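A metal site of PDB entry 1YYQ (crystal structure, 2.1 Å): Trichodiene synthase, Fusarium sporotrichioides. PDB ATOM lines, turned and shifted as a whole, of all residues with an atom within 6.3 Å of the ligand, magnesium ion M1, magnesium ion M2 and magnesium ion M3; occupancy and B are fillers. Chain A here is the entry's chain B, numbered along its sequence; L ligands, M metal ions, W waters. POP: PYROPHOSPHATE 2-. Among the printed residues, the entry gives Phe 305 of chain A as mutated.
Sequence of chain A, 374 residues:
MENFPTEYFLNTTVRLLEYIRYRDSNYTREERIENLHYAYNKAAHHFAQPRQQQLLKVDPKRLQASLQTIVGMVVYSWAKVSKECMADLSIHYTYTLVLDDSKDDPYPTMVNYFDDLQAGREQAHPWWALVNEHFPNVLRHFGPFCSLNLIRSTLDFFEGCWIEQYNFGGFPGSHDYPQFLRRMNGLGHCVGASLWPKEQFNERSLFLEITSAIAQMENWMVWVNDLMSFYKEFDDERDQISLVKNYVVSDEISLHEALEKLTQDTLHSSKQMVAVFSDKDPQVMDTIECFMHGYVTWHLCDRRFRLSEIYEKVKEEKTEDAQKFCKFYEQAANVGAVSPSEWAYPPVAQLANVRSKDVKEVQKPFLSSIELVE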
ATOM      1  N   LEU A  97      -3.184  13.621   9.871  1.00  0.00           N
ATOM      2  CA  LEU A  97      -3.027  14.707   8.918  1.00  0.00           C
ATOM      3  C   LEU A  97      -3.320  14.211   7.501  1.00  0.00           C
ATOM      4  O   LEU A  97      -3.956  14.908   6.713  1.00  0.00           O
ATOM      5  CB  LEU A  97      -1.613  15.299   8.949  1.00  0.00           C
ATOM      6  CG  LEU A  97      -1.534  16.696   8.320  1.00  0.00           C
ATOM      7  CD1 LEU A  97      -2.268  17.664   9.223  1.00  0.00           C
ATOM      8  CD2 LEU A  97      -0.092  17.148   8.146  1.00  0.00           C
ATOM      9  N   ASP A 100      -6.809  14.015   7.122  1.00  0.00           N
ATOM     10  CA  ASP A 100      -7.313  15.386   7.191  1.00  0.00           C
ATOM     11  C   ASP A 100      -7.468  16.120   5.864  1.00  0.00           C
ATOM     12  O   ASP A 100      -8.332  16.977   5.717  1.00  0.00           O
ATOM     13  CB  ASP A 100      -6.427  16.214   8.130  1.00  0.00           C
ATOM     14  CG  ASP A 100      -6.992  17.586   8.402  1.00  0.00           C
ATOM     15  OD1 ASP A 100      -6.517  18.568   7.769  1.00  0.00           O
ATOM     16  OD2 ASP A 100      -7.922  17.695   9.236  1.00  0.00           O
ATOM     17  N   ASP A 101      -6.610  15.783   4.892  1.00  0.00           N
ATOM     18  CA  ASP A 101      -6.661  16.421   3.585  1.00  0.00           C
ATOM     19  C   ASP A 101      -7.231  15.497   2.516  1.00  0.00           C
ATOM     20  O   ASP A 101      -7.336  15.873   1.345  1.00  0.00           O
ATOM     21  CB  ASP A 101      -5.253  16.849   3.129  1.00  0.00           C
ATOM     22  CG  ASP A 101      -4.604  17.840   4.059  1.00  0.00           C
ATOM     23  OD1 ASP A 101      -5.283  18.785   4.537  1.00  0.00           O
ATOM     24  OD2 ASP A 101      -3.388  17.679   4.303  1.00  0.00           O
ATOM     25  N   PHE A 157     -12.492  12.279  15.259  1.00  0.00           N
ATOM     26  CA  PHE A 157     -11.814  12.855  14.109  1.00  0.00           C
ATOM     27  C   PHE A 157     -12.193  12.104  12.841  1.00  0.00           C
ATOM     28  O   PHE A 157     -12.470  12.723  11.812  1.00  0.00           O
ATOM     29  CB  PHE A 157     -10.295  12.774  14.322  1.00  0.00           C
ATOM     30  CG  PHE A 157      -9.498  13.260  13.145  1.00  0.00           C
ATOM     31  CD1 PHE A 157      -9.469  14.605  12.819  1.00  0.00           C
ATOM     32  CD2 PHE A 157      -8.791  12.362  12.356  1.00  0.00           C
ATOM     33  CE1 PHE A 157      -8.756  15.049  11.708  1.00  0.00           C
ATOM     34  CE2 PHE A 157      -8.081  12.797  11.243  1.00  0.00           C
ATOM     35  CZ  PHE A 157      -8.064  14.144  10.925  1.00  0.00           C
ATOM     36  N   CYS A 161     -13.947  13.848   9.535  1.00  0.00           N
ATOM     37  CA  CYS A 161     -13.451  13.852   8.162  1.00  0.00           C
ATOM     38  C   CYS A 161     -14.509  13.237   7.237  1.00  0.00           C
ATOM     39  O   CYS A 161     -14.560  13.560   6.044  1.00  0.00           O
ATOM     40  CB  CYS A 161     -12.152  13.045   8.061  1.00  0.00           C
ATOM     41  SG  CYS A 161     -10.736  13.791   8.933  1.00  0.00           S
ATOM     42  N   GLU A 164     -17.130  16.047   6.613  1.00  0.00           N
ATOM     43  CA  GLU A 164     -16.551  17.030   5.696  1.00  0.00           C
ATOM     44  C   GLU A 164     -16.608  16.592   4.237  1.00  0.00           C
ATOM     45  O   GLU A 164     -16.596  17.435   3.334  1.00  0.00           O
ATOM     46  CB  GLU A 164     -15.101  17.329   6.073  1.00  0.00           C
ATOM     47  CG  GLU A 164     -14.936  17.940   7.456  1.00  0.00           C
ATOM     48  CD  GLU A 164     -13.486  18.208   7.830  1.00  0.00           C
ATOM     49  OE1 GLU A 164     -12.586  17.499   7.334  1.00  0.00           O
ATOM     50  OE2 GLU A 164     -13.255  19.138   8.626  1.00  0.00           O
ATOM     51  N   ARG A 182     -16.466  21.271  14.502  1.00  0.00           N
ATOM     52  CA  ARG A 182     -15.118  21.636  14.898  1.00  0.00           C
ATOM     53  C   ARG A 182     -14.611  20.735  16.026  1.00  0.00           C
ATOM     54  O   ARG A 182     -13.465  20.275  15.990  1.00  0.00           O
ATOM     55  CB  ARG A 182     -15.050  23.111  15.318  1.00  0.00           C
ATOM     56  CG  ARG A 182     -13.618  23.633  15.535  1.00  0.00           C
ATOM     57  CD  ARG A 182     -12.699  23.122  14.438  1.00  0.00           C
ATOM     58  NE  ARG A 182     -11.384  23.773  14.468  1.00  0.00           N
ATOM     59  CZ  ARG A 182     -10.313  23.331  13.807  1.00  0.00           C
ATOM     60  NH1 ARG A 182     -10.401  22.223  13.075  1.00  0.00           N
ATOM     61  NH2 ARG A 182      -9.169  23.990  13.884  1.00  0.00           N
ATOM     62  N   ASN A 185     -13.842  17.244  14.450  1.00  0.00           N
ATOM     63  CA  ASN A 185     -12.595  17.108  13.692  1.00  0.00           C
ATOM     64  C   ASN A 185     -11.382  17.736  14.359  1.00  0.00           C
ATOM     65  O   ASN A 185     -10.282  17.708  13.811  1.00  0.00           O
ATOM     66  CB  ASN A 185     -12.754  17.766  12.325  1.00  0.00           C
ATOM     67  CG  ASN A 185     -12.961  19.271  12.419  1.00  0.00           C
ATOM     68  OD1 ASN A 185     -12.370  19.954  13.271  1.00  0.00           O
ATOM     69  ND2 ASN A 185     -13.810  19.811  11.544  1.00  0.00           N
ATOM     70  N   GLY A 186     -11.576  18.292  15.551  1.00  0.00           N
ATOM     71  CA  GLY A 186     -10.491  18.964  16.228  1.00  0.00           C
ATOM     72  C   GLY A 186      -9.369  18.189  16.874  1.00  0.00           C
ATOM     73  O   GLY A 186      -8.304  18.757  17.107  1.00  0.00           O
ATOM     74  N   VAL A 222      -8.017  24.326  18.910  1.00  0.00           N
ATOM     75  CA  VAL A 222      -8.715  24.349  17.630  1.00  0.00           C
ATOM     76  C   VAL A 222      -8.900  25.763  17.083  1.00  0.00           C
ATOM     77  O   VAL A 222      -8.671  26.027  15.901  1.00  0.00           O
ATOM     78  CB  VAL A 222     -10.106  23.656  17.720  1.00  0.00           C
ATOM     79  CG1 VAL A 222      -9.928  22.180  18.039  1.00  0.00           C
ATOM     80  CG2 VAL A 222     -10.977  24.328  18.784  1.00  0.00           C
ATOM     81  N   ASN A 225      -5.817  27.383  15.613  1.00  0.00           N
ATOM     82  CA  ASN A 225      -5.546  26.884  14.271  1.00  0.00           C
ATOM     83  C   ASN A 225      -6.548  27.458  13.273  1.00  0.00           C
ATOM     84  O   ASN A 225      -6.194  27.734  12.128  1.00  0.00           O
ATOM     85  CB  ASN A 225      -5.586  25.355  14.230  1.00  0.00           C
ATOM     86  CG  ASN A 225      -5.523  24.814  12.805  1.00  0.00           C
ATOM     87  OD1 ASN A 225      -6.550  24.670  12.145  1.00  0.00           O
ATOM     88  ND2 ASN A 225      -4.319  24.532  12.334  1.00  0.00           N
ATOM     89  N   ASP A 226      -7.797  27.633  13.700  1.00  0.00           N
ATOM     90  CA  ASP A 226      -8.781  28.196  12.790  1.00  0.00           C
ATOM     91  C   ASP A 226      -8.330  29.575  12.336  1.00  0.00           C
ATOM     92  O   ASP A 226      -8.461  29.937  11.167  1.00  0.00           O
ATOM     93  CB  ASP A 226     -10.157  28.277  13.474  1.00  0.00           C
ATOM     94  CG  ASP A 226     -10.891  26.942  13.477  1.00  0.00           C
ATOM     95  OD1 ASP A 226     -10.889  26.267  12.427  1.00  0.00           O
ATOM     96  OD2 ASP A 226     -11.466  26.568  14.518  1.00  0.00           O
ATOM     97  N   SER A 229      -4.521  29.145  10.540  1.00  0.00           N
ATOM     98  CA  SER A 229      -4.614  28.417   9.281  1.00  0.00           C
ATOM     99  C   SER A 229      -5.676  29.026   8.354  1.00  0.00           C
ATOM    100  O   SER A 229      -5.970  28.466   7.295  1.00  0.00           O
ATOM    101  CB  SER A 229      -4.957  26.941   9.526  1.00  0.00           C
ATOM    102  OG  SER A 229      -6.323  26.760   9.831  1.00  0.00           O
ATOM    103  N   PHE A 230      -6.232  30.161   8.760  1.00  0.00           N
ATOM    104  CA  PHE A 230      -7.254  30.813   7.942  1.00  0.00           C
ATOM    105  C   PHE A 230      -6.717  31.183   6.575  1.00  0.00           C
ATOM    106  O   PHE A 230      -7.477  31.302   5.621  1.00  0.00           O
ATOM    107  CB  PHE A 230      -7.768  32.072   8.644  1.00  0.00           C
ATOM    108  CG  PHE A 230      -8.820  32.813   7.848  1.00  0.00           C
ATOM    109  CD1 PHE A 230      -9.986  32.167   7.442  1.00  0.00           C
ATOM    110  CD2 PHE A 230      -8.640  34.150   7.512  1.00  0.00           C
ATOM    111  CE1 PHE A 230     -10.967  32.845   6.712  1.00  0.00           C
ATOM    112  CE2 PHE A 230      -9.609  34.835   6.785  1.00  0.00           C
ATOM    113  CZ  PHE A 230     -10.775  34.188   6.380  1.00  0.00           C
ATOM    114  N   LYS A 232      -4.041  29.439   4.639  1.00  0.00           N
ATOM    115  CA  LYS A 232      -3.860  28.283   3.759  1.00  0.00           C
ATOM    116  C   LYS A 232      -5.226  27.740   3.381  1.00  0.00           C
ATOM    117  O   LYS A 232      -5.432  27.216   2.278  1.00  0.00           O
ATOM    118  CB  LYS A 232      -2.995  27.196   4.426  1.00  0.00           C
ATOM    119  CG  LYS A 232      -3.646  26.408   5.541  1.00  0.00           C
ATOM    120  CD  LYS A 232      -4.332  25.145   5.011  1.00  0.00           C
ATOM    121  CE  LYS A 232      -4.756  24.215   6.154  1.00  0.00           C
ATOM    122  NZ  LYS A 232      -5.366  22.931   5.685  1.00  0.00           N
ATOM    123  N   GLU A 233      -6.165  27.856   4.307  1.00  0.00           N
ATOM    124  CA  GLU A 233      -7.545  27.449   4.074  1.00  0.00           C
ATOM    125  C   GLU A 233      -8.129  28.739   3.539  1.00  0.00           C
ATOM    126  O   GLU A 233      -7.672  29.818   3.923  1.00  0.00           O
ATOM    127  CB  GLU A 233      -8.240  27.088   5.397  1.00  0.00           C
ATOM    128  CG  GLU A 233      -7.588  25.958   6.167  1.00  0.00           C
ATOM    129  CD  GLU A 233      -8.277  25.649   7.486  1.00  0.00           C
ATOM    130  OE1 GLU A 233      -7.967  24.592   8.083  1.00  0.00           O
ATOM    131  OE2 GLU A 233      -9.131  26.451   7.921  1.00  0.00           O
ATOM    132  N   ARG A 238     -10.498  21.319  -0.450  1.00  0.00           N
ATOM    133  CA  ARG A 238     -10.711  20.361   0.636  1.00  0.00           C
ATOM    134  C   ARG A 238     -11.172  21.052   1.901  1.00  0.00           C
ATOM    135  O   ARG A 238     -11.874  20.456   2.729  1.00  0.00           O
ATOM    136  CB  ARG A 238      -9.425  19.577   0.962  1.00  0.00           C
ATOM    137  CG  ARG A 238      -9.552  18.673   2.202  1.00  0.00           C
ATOM    138  CD  ARG A 238     -10.673  17.637   2.021  1.00  0.00           C
ATOM    139  NE  ARG A 238     -10.832  16.711   3.146  1.00  0.00           N
ATOM    140  CZ  ARG A 238     -11.365  17.014   4.331  1.00  0.00           C
ATOM    141  NH1 ARG A 238     -11.794  18.249   4.574  1.00  0.00           N
ATOM    142  NH2 ARG A 238     -11.477  16.079   5.259  1.00  0.00           N
ATOM    143  N   ASP A 239     -10.761  22.296   2.081  1.00  0.00           N
ATOM    144  CA  ASP A 239     -11.175  23.023   3.248  1.00  0.00           C
ATOM    145  C   ASP A 239     -12.499  23.697   2.890  1.00  0.00           C
ATOM    146  O   ASP A 239     -13.449  22.992   2.540  1.00  0.00           O
ATOM    147  CB  ASP A 239     -10.067  24.008   3.672  1.00  0.00           C
ATOM    148  CG  ASP A 239      -8.750  23.289   4.002  1.00  0.00           C
ATOM    149  OD1 ASP A 239      -8.749  22.034   4.064  1.00  0.00           O
ATOM    150  OD2 ASP A 239      -7.709  23.954   4.197  1.00  0.00           O
ATOM    151  N   TRP A 298       4.931  26.925  15.493  1.00  0.00           N
ATOM    152  CA  TRP A 298       4.694  25.962  14.420  1.00  0.00           C
ATOM    153  C   TRP A 298       3.821  26.534  13.291  1.00  0.00           C
ATOM    154  O   TRP A 298       4.128  26.366  12.108  1.00  0.00           O
ATOM    155  CB  TRP A 298       4.055  24.706  15.010  1.00  0.00           C
ATOM    156  CG  TRP A 298       3.640  23.708  13.999  1.00  0.00           C
ATOM    157  CD1 TRP A 298       4.460  23.012  13.147  1.00  0.00           C
ATOM    158  CD2 TRP A 298       2.309  23.261  13.734  1.00  0.00           C
ATOM    159  NE1 TRP A 298       3.707  22.158  12.378  1.00  0.00           N
ATOM    160  CE2 TRP A 298       2.382  22.297  12.717  1.00  0.00           C
ATOM    161  CE3 TRP A 298       1.050  23.589  14.267  1.00  0.00           C
ATOM    162  CZ2 TRP A 298       1.250  21.639  12.206  1.00  0.00           C
ATOM    163  CZ3 TRP A 298      -0.079  22.949  13.769  1.00  0.00           C
ATOM    164  CH2 TRP A 298       0.024  21.977  12.749  1.00  0.00           C
ATOM    165  N   HIS A 299       2.721  27.194  13.663  1.00  0.00           N
ATOM    166  CA  HIS A 299       1.830  27.778  12.667  1.00  0.00           C
ATOM    167  C   HIS A 299       2.537  28.866  11.849  1.00  0.00           C
ATOM    168  O   HIS A 299       2.307  28.990  10.637  1.00  0.00           O
ATOM    169  CB  HIS A 299       0.594  28.357  13.347  1.00  0.00           C
ATOM    170  CG  HIS A 299      -0.398  27.332  13.788  1.00  0.00           C
ATOM    171  ND1 HIS A 299      -1.280  26.733  12.914  1.00  0.00           N
ATOM    172  CD2 HIS A 299      -0.623  26.767  14.993  1.00  0.00           C
ATOM    173  CE1 HIS A 299      -2.013  25.848  13.578  1.00  0.00           C
ATOM    174  NE2 HIS A 299      -1.627  25.851  14.846  1.00  0.00           N
ATOM    175  N   ARG A 304       3.023  24.213   5.627  1.00  0.00           N
ATOM    176  CA  ARG A 304       1.598  23.908   5.486  1.00  0.00           C
ATOM    177  C   ARG A 304       0.697  25.132   5.574  1.00  0.00           C
ATOM    178  O   ARG A 304      -0.308  25.222   4.871  1.00  0.00           O
ATOM    179  CB  ARG A 304       1.146  22.886   6.539  1.00  0.00           C
ATOM    180  CG  ARG A 304      -0.330  22.474   6.425  1.00  0.00           C
ATOM    181  CD  ARG A 304      -0.788  21.640   7.610  1.00  0.00           C
ATOM    182  NE  ARG A 304      -2.190  21.221   7.537  1.00  0.00           N
ATOM    183  CZ  ARG A 304      -2.660  20.290   6.705  1.00  0.00           C
ATOM    184  NH1 ARG A 304      -1.853  19.683   5.848  1.00  0.00           N
ATOM    185  NH2 ARG A 304      -3.949  19.968   6.736  1.00  0.00           N
ATOM    186  N   PHE A 305       1.052  26.083   6.418  1.00  0.00           N
ATOM    187  CA  PHE A 305       0.224  27.271   6.597  1.00  0.00           C
ATOM    188  C   PHE A 305       0.648  28.472   5.762  1.00  0.00           C
ATOM    189  O   PHE A 305       0.000  29.523   5.779  1.00  0.00           O
ATOM    190  CB  PHE A 305       0.172  27.611   8.067  1.00  0.00           C
ATOM    191  CG  PHE A 305      -0.244  26.447   8.918  1.00  0.00           C
ATOM    192  CD1 PHE A 305       0.660  25.822   9.768  1.00  0.00           C
ATOM    193  CD2 PHE A 305      -1.540  25.939   8.824  1.00  0.00           C
ATOM    194  CE1 PHE A 305       0.284  24.698  10.509  1.00  0.00           C
ATOM    195  CE2 PHE A 305      -1.925  24.818   9.563  1.00  0.00           C
ATOM    196  CZ  PHE A 305      -1.006  24.200  10.407  1.00  0.00           C
HETATM  197  P1  POP L   1      -7.678  21.348  10.687  1.00  0.00           P
HETATM  198  O1  POP L   1      -8.264  22.752  10.694  1.00  0.00           O
HETATM  199  O2  POP L   1      -8.354  20.545   9.632  1.00  0.00           O
HETATM  200  O3  POP L   1      -7.828  20.668  12.006  1.00  0.00           O
HETATM  201  O   POP L   1      -6.051  21.527  10.632  1.00  0.00           O
HETATM  202  P2  POP L   1      -5.229  22.288   9.407  1.00  0.00           P
HETATM  203  O4  POP L   1      -5.621  23.793   9.375  1.00  0.00           O
HETATM  204  O5  POP L   1      -5.643  21.558   8.130  1.00  0.00           O
HETATM  205  O6  POP L   1      -3.849  22.127   9.812  1.00  0.00           O
HETATM  206 MG    MG M   1      -7.505  24.595  10.166  1.00  0.00          MG
HETATM  207 MG    MG M   2      -7.552  20.408   7.631  1.00  0.00          MG
HETATM  208 MG    MG M   3      -9.467  18.870   9.419  1.00  0.00          MG
HETATM  209  O   HOH W   1      -7.132  20.352   5.708  1.00  0.00           O
HETATM  210  O   HOH W   2      -8.419  22.195   7.055  1.00  0.00           O
HETATM  211  O   HOH W   3      -9.193  25.875  10.580  1.00  0.00           O
HETATM  212  O   HOH W   4     -10.734  22.746   9.682  1.00  0.00           O
HETATM  213  O   HOH W   5     -11.020  20.188   9.468  1.00  0.00           O
HETATM  214  O   HOH W   6     -10.759  17.314   9.293  1.00  0.00           O
HETATM  215  O   HOH W   7      -9.274  19.072   7.176  1.00  0.00           O
HETATM  216  O   HOH W   8      -9.346  18.577  11.449  1.00  0.00           O
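O6 of the ligand is in salt-bridge range of NE of Arg 304 (3.0 Å).
NZ of Lys 232 sits close to O5 of the ligand.
The guanidinium group of Arg 182 lies within salt-bridge range of an oxygen (O3) of the ligand (3.2 Å).
The backbone carbonyl oxygen (O) of Asp 100 sits at hydrogen-bond distance from the guanidinium group (NH2) of Arg 238, at 3.3 Å.
The side-chain carboxylate of Glu 233 sits close to the side-chain amino group of Lys 232 (3.9 Å).
The guanidinium group of Arg 182 lies close to the side-chain amide oxygen of Asn 225 (3.2 Å).
The side-chain carboxylate (OD1) of Asp 101 is in salt-bridge range of the guanidinium group (NH2) of Arg 304, 2.8 Å away.
The side-chain carboxylate (OD2) of Asp 239 lies within salt-bridge range of the side-chain amino group (NZ) of Lys 232, at 3.0 Å.
O of Arg 182 lies close to OD1 of Asn 185, at 2.9 Å.
The side-chain carboxylate (OE2) of Glu 164 is in hydrogen-bond range of the side-chain amide nitrogen (ND2) of Asn 185 (3.0 Å).
The guanidinium group (NH2) of Arg 238 is in salt-bridge range of the side-chain carboxylate (OE1) of Glu 164 (2.7 Å).
Phe 305 touches the ligand.
Hydrophobic or aromatic side chains that line the ligand: Phe 305.
Within 4 Å of the ligand: Asp 100, Arg 182, Asn 225, Ser 229, Lys 232, Glu 233, Arg 304 and Phe 305.
Along chain A the residues within 4 Å of the ligand span positions 100 to 305.
Within 4 Å of magnesium ion M1: Asn 225, Ser 229 and Glu 233.
Along chain A the residues within 4 Å of magnesium ion M1 span positions 225 to 233.
Lys 232 touches magnesium ion M2.
NH2 of Arg 304 touches magnesium ion M2, at 3.7 Å.
Within 4 Å of magnesium ion M2: Asp 100, Lys 232 and Arg 304.
Residues that only touch magnesium ion M3: Glu 164 (3.9 Å).
Two residues have an atom within 4 Å of magnesium ion M3: Asp 100 and Glu 164.
Magnesium ion M1 is bound by an oxygen (O1) of the ligand (2.1 Å).
Magnesium ion M1 is bound by OE1 of Glu 233 (2.1 Å).
Water W3 is bound to magnesium ion M1, 2.2 Å away.
An oxygen (O4) of the ligand is bound to magnesium ion M1.
Magnesium ion M1 is bound by OD1 of Asn 225 (2.2 Å).
Magnesium ion M1 is bound by OG of Ser 229, at 2.5 Å.
Magnesium ion M1 has six donor atoms within binding distance.
Magnesium ion M2 is bound by water W1 (2.0 Å), water W2 (2.1 Å), OD1 of Asp 100 (2.1 Å), O2 of the ligand (2.2 Å), water W7 (2.2 Å) and O5 of the ligand (2.3 Å).
Magnesium ion M2 has six donor atoms within binding distance.
Magnesium ion M3 is bound by OD2 of Asp 100, O2 of the ligand, water W6, water W5, water W8 and water W7.
Water W3 bridges the side-chain carboxylate (OD1) of Asp 226 and the side-chain carboxylate (OE2) of Glu 233.
Water W2 lies within hydrogen-bond range of OD1 of Asp 239 and NZ of Lys 232.
Water W1 lies within hydrogen-bond range of the side-chain carboxylate (OD1) of Asp 101 (2.7 Å), the side-chain carboxylate (OD1) of Asp 239 (2.9 Å), the side-chain amino group (NZ) of Lys 232 (3.1 Å) and the guanidinium group (NH2) of Arg 304 (3.4 Å).
Water W5 bridges OE2 of Glu 164 (2.6 Å) and ND2 of Asn 185 (3.5 Å).
Water W8 lies within hydrogen-bond range of an oxygen (O3) of the ligand (2.6 Å) and the backbone carbonyl oxygen of Asn 185 (2.7 Å).
Water W6 lies within hydrogen-bond range of OE1 of Glu 164 (2.7 Å) and SG of Cys 161 (3.5 Å).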
